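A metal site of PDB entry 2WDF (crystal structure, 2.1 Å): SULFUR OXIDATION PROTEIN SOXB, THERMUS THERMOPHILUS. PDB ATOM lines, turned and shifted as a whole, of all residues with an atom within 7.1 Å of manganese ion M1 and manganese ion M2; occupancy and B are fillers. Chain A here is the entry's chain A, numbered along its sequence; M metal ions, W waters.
OD2 of Asp 36 lies within hydrogen-bond range of N of His 286 (2.9 Å). N of Asp 36 sits at hydrogen-bond distance from O of Gly 131 (2.8 Å). The backbone carbonyl oxygen (O) of His 263 sits close to the backbone NH (N) of Tyr 219 (3.4 Å). The backbone NH of Trp 164 lies within hydrogen-bond range of the side-chain carboxylate of Asp 132, 2.7 Å away. The backbone NH (N) of Leu 37 lies within hydrogen-bond range of the backbone carbonyl oxygen (O) of Asp 132, 3.3 Å away. NE2 of His 226 is in hydrogen-bond range of NE2 of His 163 (2.8 Å). A ring nitrogen (ND1) of His 38 sits at hydrogen-bond distance from the side-chain amide oxygen of Asn 136 (2.7 Å). The backbone carbonyl oxygen (O) of Arg 405 is in hydrogen-bond range of a ring nitrogen (ND1) of His 288 (2.9 Å).
Five residues have an atom within 4 Å of manganese ion M1: Asp 36, Asp 132, His 163, His 263 and His 286. The nearest printed residue that does not touch manganese ion M1 is Trp 164 (4.1 Å).
The nearest printed residue that does not touch manganese ion M2 is His 286 (4.1 Å).
Water W1 is bound to manganese ion M1 (2.2 Å). NE2 of His 263 is bound to manganese ion M1 (2.2 Å). Manganese ion M1 is bound by the side-chain carboxylate (OD2) of Asp 132 (2.2 Å). Manganese ion M1 is bound by ND1 of His 163, 2.2 Å away. Manganese ion M1 is bound by ND1 of His 286, 2.4 Å away.
Manganese ion M2 is bound by water W1 (2.0 Å), OD1 of Asp 36 (2.1 Å), OD2 of Asp 132 (2.3 Å), NE2 of His 38 (2.3 Å) and NE2 of His 288 (2.3 Å).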
ATOM      1  N   SER A  35     -28.760 -24.258  17.680  1.00  0.00           N
ATOM      2  CA  SER A  35     -27.390 -24.627  17.902  1.00  0.00           C
ATOM      3  C   SER A  35     -27.286 -25.915  18.715  1.00  0.00           C
ATOM      4  O   SER A  35     -28.222 -26.290  19.409  1.00  0.00           O
ATOM      5  CB  SER A  35     -26.668 -23.504  18.651  1.00  0.00           C
ATOM      6  OG  SER A  35     -25.266 -23.721  18.676  1.00  0.00           O
ATOM      7  N   ASP A  36     -26.140 -26.569  18.614  1.00  0.00           N
ATOM      8  CA  ASP A  36     -25.863 -27.738  19.426  1.00  0.00           C
ATOM      9  C   ASP A  36     -26.912 -28.848  19.322  1.00  0.00           C
ATOM     10  O   ASP A  36     -27.312 -29.445  20.333  1.00  0.00           O
ATOM     11  CB  ASP A  36     -25.713 -27.285  20.889  1.00  0.00           C
ATOM     12  CG  ASP A  36     -24.525 -26.352  21.085  1.00  0.00           C
ATOM     13  OD1 ASP A  36     -23.410 -26.874  21.306  1.00  0.00           O
ATOM     14  OD2 ASP A  36     -24.679 -25.113  21.026  1.00  0.00           O
ATOM     15  N   LEU A  37     -27.311 -29.142  18.087  1.00  0.00           N
ATOM     16  CA  LEU A  37     -28.260 -30.210  17.795  1.00  0.00           C
ATOM     17  C   LEU A  37     -27.636 -31.564  18.183  1.00  0.00           C
ATOM     18  O   LEU A  37     -28.331 -32.474  18.635  1.00  0.00           O
ATOM     19  CB  LEU A  37     -28.611 -30.208  16.302  1.00  0.00           C
ATOM     20  CG  LEU A  37     -29.625 -31.252  15.800  1.00  0.00           C
ATOM     21  CD1 LEU A  37     -31.023 -30.979  16.327  1.00  0.00           C
ATOM     22  CD2 LEU A  37     -29.657 -31.285  14.277  1.00  0.00           C
ATOM     23  N   HIS A  38     -26.323 -31.664  18.038  1.00  0.00           N
ATOM     24  CA  HIS A  38     -25.616 -32.913  18.384  1.00  0.00           C
ATOM     25  C   HIS A  38     -26.271 -34.126  17.728  1.00  0.00           C
ATOM     26  O   HIS A  38     -26.563 -35.118  18.371  1.00  0.00           O
ATOM     27  CB  HIS A  38     -25.472 -33.096  19.898  1.00  0.00           C
ATOM     28  CG  HIS A  38     -24.408 -32.225  20.501  1.00  0.00           C
ATOM     29  ND1 HIS A  38     -23.079 -32.609  20.549  1.00  0.00           N
ATOM     30  CD2 HIS A  38     -24.454 -30.979  21.006  1.00  0.00           C
ATOM     31  CE1 HIS A  38     -22.366 -31.634  21.094  1.00  0.00           C
ATOM     32  NE2 HIS A  38     -23.180 -30.626  21.374  1.00  0.00           N
ATOM     33  N   GLY A 130     -25.546 -22.721  15.038  1.00  0.00           N
ATOM     34  CA  GLY A 130     -24.461 -22.443  15.963  1.00  0.00           C
ATOM     35  C   GLY A 130     -23.352 -23.469  16.137  1.00  0.00           C
ATOM     36  O   GLY A 130     -22.369 -23.204  16.856  1.00  0.00           O
ATOM     37  N   GLY A 131     -23.462 -24.628  15.486  1.00  0.00           N
ATOM     38  CA  GLY A 131     -22.432 -25.650  15.565  1.00  0.00           C
ATOM     39  C   GLY A 131     -22.770 -26.835  16.461  1.00  0.00           C
ATOM     40  O   GLY A 131     -23.858 -26.873  17.055  1.00  0.00           O
ATOM     41  N   ASP A 132     -21.864 -27.797  16.562  1.00  0.00           N
ATOM     42  CA  ASP A 132     -22.119 -29.013  17.320  1.00  0.00           C
ATOM     43  C   ASP A 132     -23.358 -29.702  16.764  1.00  0.00           C
ATOM     44  O   ASP A 132     -24.213 -30.184  17.495  1.00  0.00           O
ATOM     45  CB  ASP A 132     -22.272 -28.731  18.810  1.00  0.00           C
ATOM     46  CG  ASP A 132     -20.945 -28.713  19.522  1.00  0.00           C
ATOM     47  OD1 ASP A 132     -19.922 -28.829  18.812  1.00  0.00           O
ATOM     48  OD2 ASP A 132     -20.911 -28.483  20.754  1.00  0.00           O
ATOM     49  N   THR A 133     -23.414 -29.729  15.435  1.00  0.00           N
ATOM     50  CA  THR A 133     -24.516 -30.318  14.685  1.00  0.00           C
ATOM     51  C   THR A 133     -24.270 -31.750  14.186  1.00  0.00           C
ATOM     52  O   THR A 133     -25.128 -32.620  14.282  1.00  0.00           O
ATOM     53  CB  THR A 133     -24.803 -29.426  13.453  1.00  0.00           C
ATOM     54  OG1 THR A 133     -24.802 -28.053  13.857  1.00  0.00           O
ATOM     55  CG2 THR A 133     -26.123 -29.775  12.810  1.00  0.00           C
ATOM     56  N   ASN A 136     -22.326 -36.954  17.537  1.00  0.00           N
ATOM     57  CA  ASN A 136     -22.965 -37.421  18.774  1.00  0.00           C
ATOM     58  C   ASN A 136     -24.392 -37.976  18.719  1.00  0.00           C
ATOM     59  O   ASN A 136     -25.218 -37.669  19.575  1.00  0.00           O
ATOM     60  CB  ASN A 136     -22.816 -36.360  19.865  1.00  0.00           C
ATOM     61  CG  ASN A 136     -21.452 -35.684  19.833  1.00  0.00           C
ATOM     62  OD1 ASN A 136     -21.343 -34.486  19.585  1.00  0.00           O
ATOM     63  ND2 ASN A 136     -20.391 -36.473  20.015  1.00  0.00           N
ATOM     64  N   SER A 162     -18.502 -24.134  14.229  1.00  0.00           N
ATOM     65  CA  SER A 162     -18.189 -25.494  14.657  1.00  0.00           C
ATOM     66  C   SER A 162     -17.539 -25.664  16.018  1.00  0.00           C
ATOM     67  O   SER A 162     -16.991 -24.723  16.605  1.00  0.00           O
ATOM     68  CB  SER A 162     -17.239 -26.121  13.630  1.00  0.00           C
ATOM     69  OG  SER A 162     -15.951 -25.510  13.733  1.00  0.00           O
ATOM     70  N   HIS A 163     -17.546 -26.919  16.463  1.00  0.00           N
ATOM     71  CA  HIS A 163     -16.845 -27.366  17.651  1.00  0.00           C
ATOM     72  C   HIS A 163     -16.580 -28.871  17.505  1.00  0.00           C
ATOM     73  O   HIS A 163     -15.538 -29.272  16.979  1.00  0.00           O
ATOM     74  CB  HIS A 163     -17.563 -27.014  18.958  1.00  0.00           C
ATOM     75  CG  HIS A 163     -16.958 -27.685  20.171  1.00  0.00           C
ATOM     76  ND1 HIS A 163     -17.611 -27.760  21.380  1.00  0.00           N
ATOM     77  CD2 HIS A 163     -15.796 -28.359  20.337  1.00  0.00           C
ATOM     78  CE1 HIS A 163     -16.878 -28.444  22.243  1.00  0.00           C
ATOM     79  NE2 HIS A 163     -15.767 -28.813  21.640  1.00  0.00           N
ATOM     80  N   TRP A 164     -17.554 -29.698  17.906  1.00  0.00           N
ATOM     81  CA  TRP A 164     -17.432 -31.168  17.843  1.00  0.00           C
ATOM     82  C   TRP A 164     -17.269 -31.726  16.435  1.00  0.00           C
ATOM     83  O   TRP A 164     -16.824 -32.870  16.260  1.00  0.00           O
ATOM     84  CB  TRP A 164     -18.596 -31.886  18.556  1.00  0.00           C
ATOM     85  CG  TRP A 164     -18.436 -31.915  20.049  1.00  0.00           C
ATOM     86  CD1 TRP A 164     -18.719 -30.906  20.918  1.00  0.00           C
ATOM     87  CD2 TRP A 164     -17.887 -32.976  20.845  1.00  0.00           C
ATOM     88  NE1 TRP A 164     -18.412 -31.290  22.202  1.00  0.00           N
ATOM     89  CE2 TRP A 164     -17.874 -32.541  22.175  1.00  0.00           C
ATOM     90  CE3 TRP A 164     -17.364 -34.241  20.536  1.00  0.00           C
ATOM     91  CZ2 TRP A 164     -17.366 -33.322  23.211  1.00  0.00           C
ATOM     92  CZ3 TRP A 164     -16.890 -35.025  21.559  1.00  0.00           C
ATOM     93  CH2 TRP A 164     -16.902 -34.575  22.878  1.00  0.00           C
ATOM     94  N   TYR A 219     -15.329 -22.792  18.440  1.00  0.00           N
ATOM     95  CA  TYR A 219     -14.835 -23.046  19.812  1.00  0.00           C
ATOM     96  C   TYR A 219     -13.311 -22.963  19.830  1.00  0.00           C
ATOM     97  O   TYR A 219     -12.627 -23.667  19.087  1.00  0.00           O
ATOM     98  CB  TYR A 219     -15.301 -24.428  20.296  1.00  0.00           C
ATOM     99  CG  TYR A 219     -15.025 -24.698  21.764  1.00  0.00           C
ATOM    100  CD1 TYR A 219     -15.536 -23.873  22.754  1.00  0.00           C
ATOM    101  CD2 TYR A 219     -14.244 -25.772  22.151  1.00  0.00           C
ATOM    102  CE1 TYR A 219     -15.268 -24.109  24.096  1.00  0.00           C
ATOM    103  CE2 TYR A 219     -13.973 -26.022  23.496  1.00  0.00           C
ATOM    104  CZ  TYR A 219     -14.502 -25.186  24.456  1.00  0.00           C
ATOM    105  OH  TYR A 219     -14.306 -25.484  25.792  1.00  0.00           O
ATOM    106  N   HIS A 226     -10.123 -32.295  22.763  1.00  0.00           N
ATOM    107  CA  HIS A 226     -10.227 -33.510  21.972  1.00  0.00           C
ATOM    108  C   HIS A 226      -8.840 -33.977  21.539  1.00  0.00           C
ATOM    109  O   HIS A 226      -7.865 -33.255  21.704  1.00  0.00           O
ATOM    110  CB  HIS A 226     -11.126 -33.258  20.766  1.00  0.00           C
ATOM    111  CG  HIS A 226     -12.344 -32.445  21.095  1.00  0.00           C
ATOM    112  ND1 HIS A 226     -13.488 -33.005  21.616  1.00  0.00           N
ATOM    113  CD2 HIS A 226     -12.573 -31.115  21.015  1.00  0.00           C
ATOM    114  CE1 HIS A 226     -14.382 -32.051  21.834  1.00  0.00           C
ATOM    115  NE2 HIS A 226     -13.849 -30.899  21.477  1.00  0.00           N
ATOM    116  N   HIS A 263     -19.539 -19.948  18.899  1.00  0.00           N
ATOM    117  CA  HIS A 263     -19.411 -21.233  19.580  1.00  0.00           C
ATOM    118  C   HIS A 263     -18.320 -21.162  20.629  1.00  0.00           C
ATOM    119  O   HIS A 263     -17.637 -22.163  20.914  1.00  0.00           O
ATOM    120  CB  HIS A 263     -19.182 -22.428  18.637  1.00  0.00           C
ATOM    121  CG  HIS A 263     -19.653 -23.719  19.223  1.00  0.00           C
ATOM    122  ND1 HIS A 263     -20.846 -24.316  18.850  1.00  0.00           N
ATOM    123  CD2 HIS A 263     -19.202 -24.432  20.280  1.00  0.00           C
ATOM    124  CE1 HIS A 263     -21.046 -25.390  19.594  1.00  0.00           C
ATOM    125  NE2 HIS A 263     -20.060 -25.480  20.470  1.00  0.00           N
ATOM    126  N   GLY A 285     -23.755 -20.271  21.190  1.00  0.00           N
ATOM    127  CA  GLY A 285     -23.826 -21.726  21.237  1.00  0.00           C
ATOM    128  C   GLY A 285     -22.902 -22.254  22.326  1.00  0.00           C
ATOM    129  O   GLY A 285     -22.482 -21.505  23.212  1.00  0.00           O
ATOM    130  N   HIS A 286     -22.634 -23.568  22.288  1.00  0.00           N
ATOM    131  CA  HIS A 286     -21.714 -24.259  23.199  1.00  0.00           C
ATOM    132  C   HIS A 286     -22.153 -24.584  24.623  1.00  0.00           C
ATOM    133  O   HIS A 286     -21.903 -25.689  25.114  1.00  0.00           O
ATOM    134  CB  HIS A 286     -20.362 -23.568  23.268  1.00  0.00           C
ATOM    135  CG  HIS A 286     -19.337 -24.349  24.027  1.00  0.00           C
ATOM    136  ND1 HIS A 286     -18.910 -25.601  23.616  1.00  0.00           N
ATOM    137  CD2 HIS A 286     -18.708 -24.094  25.200  1.00  0.00           C
ATOM    138  CE1 HIS A 286     -18.025 -26.062  24.496  1.00  0.00           C
ATOM    139  NE2 HIS A 286     -17.887 -25.175  25.463  1.00  0.00           N
ATOM    140  N   THR A 287     -22.712 -23.603  25.322  1.00  0.00           N
ATOM    141  CA  THR A 287     -23.119 -23.783  26.702  1.00  0.00           C
ATOM    142  C   THR A 287     -24.510 -24.381  26.893  1.00  0.00           C
ATOM    143  O   THR A 287     -24.891 -24.716  28.017  1.00  0.00           O
ATOM    144  CB  THR A 287     -22.867 -22.529  27.550  1.00  0.00           C
ATOM    145  OG1 THR A 287     -23.135 -21.343  26.770  1.00  0.00           O
ATOM    146  CG2 THR A 287     -21.391 -22.494  27.989  1.00  0.00           C
ATOM    147  N   HIS A 288     -25.220 -24.580  25.777  1.00  0.00           N
ATOM    148  CA  HIS A 288     -26.560 -25.188  25.763  1.00  0.00           C
ATOM    149  C   HIS A 288     -27.602 -24.405  26.569  1.00  0.00           C
ATOM    150  O   HIS A 288     -28.564 -24.966  27.102  1.00  0.00           O
ATOM    151  CB  HIS A 288     -26.492 -26.649  26.238  1.00  0.00           C
ATOM    152  CG  HIS A 288     -25.676 -27.528  25.334  1.00  0.00           C
ATOM    153  ND1 HIS A 288     -25.800 -28.904  25.327  1.00  0.00           N
ATOM    154  CD2 HIS A 288     -24.718 -27.238  24.425  1.00  0.00           C
ATOM    155  CE1 HIS A 288     -24.956 -29.418  24.459  1.00  0.00           C
ATOM    156  NE2 HIS A 288     -24.280 -28.433  23.902  1.00  0.00           N
ATOM    157  N   SER A 306     -29.757 -22.967  22.861  1.00  0.00           N
ATOM    158  CA  SER A 306     -30.324 -24.200  23.402  1.00  0.00           C
ATOM    159  C   SER A 306     -29.551 -25.417  22.884  1.00  0.00           C
ATOM    160  O   SER A 306     -28.334 -25.331  22.673  1.00  0.00           O
ATOM    161  CB  SER A 306     -31.828 -24.317  23.106  1.00  0.00           C
ATOM    162  OG  SER A 306     -32.463 -25.313  23.916  1.00  0.00           O
ATOM    163  N   ALA A 307     -30.229 -26.555  22.702  1.00  0.00           N
ATOM    164  CA  ALA A 307     -29.535 -27.765  22.284  1.00  0.00           C
ATOM    165  C   ALA A 307     -30.441 -28.936  21.928  1.00  0.00           C
ATOM    166  O   ALA A 307     -31.602 -28.982  22.315  1.00  0.00           O
ATOM    167  CB  ALA A 307     -28.592 -28.213  23.409  1.00  0.00           C
ATOM    168  N   ARG A 405     -22.336 -31.596  28.017  1.00  0.00           N
ATOM    169  CA  ARG A 405     -23.688 -31.042  28.105  1.00  0.00           C
ATOM    170  C   ARG A 405     -24.654 -31.617  27.079  1.00  0.00           C
ATOM    171  O   ARG A 405     -25.833 -31.275  27.059  1.00  0.00           O
ATOM    172  CB  ARG A 405     -23.644 -29.522  27.983  1.00  0.00           C
ATOM    173  CG  ARG A 405     -23.744 -28.801  29.333  1.00  0.00           C
ATOM    174  CD  ARG A 405     -22.533 -27.907  29.565  1.00  0.00           C
ATOM    175  NE  ARG A 405     -22.888 -26.502  29.448  1.00  0.00           N
ATOM    176  CZ  ARG A 405     -22.901 -25.645  30.461  1.00  0.00           C
ATOM    177  NH1 ARG A 405     -22.589 -26.052  31.675  1.00  0.00           N
ATOM    178  NH2 ARG A 405     -23.234 -24.376  30.257  1.00  0.00           N
ATOM    179  N   TRP A 406     -24.140 -32.494  26.206  1.00  0.00           N
ATOM    180  CA  TRP A 406     -25.002 -33.132  25.228  1.00  0.00           C
ATOM    181  C   TRP A 406     -25.487 -34.460  25.793  1.00  0.00           C
ATOM    182  O   TRP A 406     -24.865 -35.011  26.691  1.00  0.00           O
ATOM    183  CB  TRP A 406     -24.302 -33.344  23.869  1.00  0.00           C
ATOM    184  CG  TRP A 406     -22.890 -33.869  23.907  1.00  0.00           C
ATOM    185  CD1 TRP A 406     -21.744 -33.136  23.905  1.00  0.00           C
ATOM    186  CD2 TRP A 406     -22.474 -35.239  23.717  1.00  0.00           C
ATOM    187  NE1 TRP A 406     -20.650 -33.953  23.759  1.00  0.00           N
ATOM    188  CE2 TRP A 406     -21.076 -35.253  23.663  1.00  0.00           C
ATOM    189  CE3 TRP A 406     -23.163 -36.457  23.673  1.00  0.00           C
ATOM    190  CZ2 TRP A 406     -20.336 -36.434  23.536  1.00  0.00           C
ATOM    191  CZ3 TRP A 406     -22.441 -37.638  23.529  1.00  0.00           C
ATOM    192  CH2 TRP A 406     -21.039 -37.608  23.470  1.00  0.00           C
HETATM  193 MN    MN M   1     -19.653 -27.089  21.920  1.00  0.00          MN
HETATM  194 MN    MN M   2     -22.629 -28.587  22.273  1.00  0.00          MN
HETATM  195  O   HOH W   1     -21.117 -27.836  23.380  1.00  0.00           O
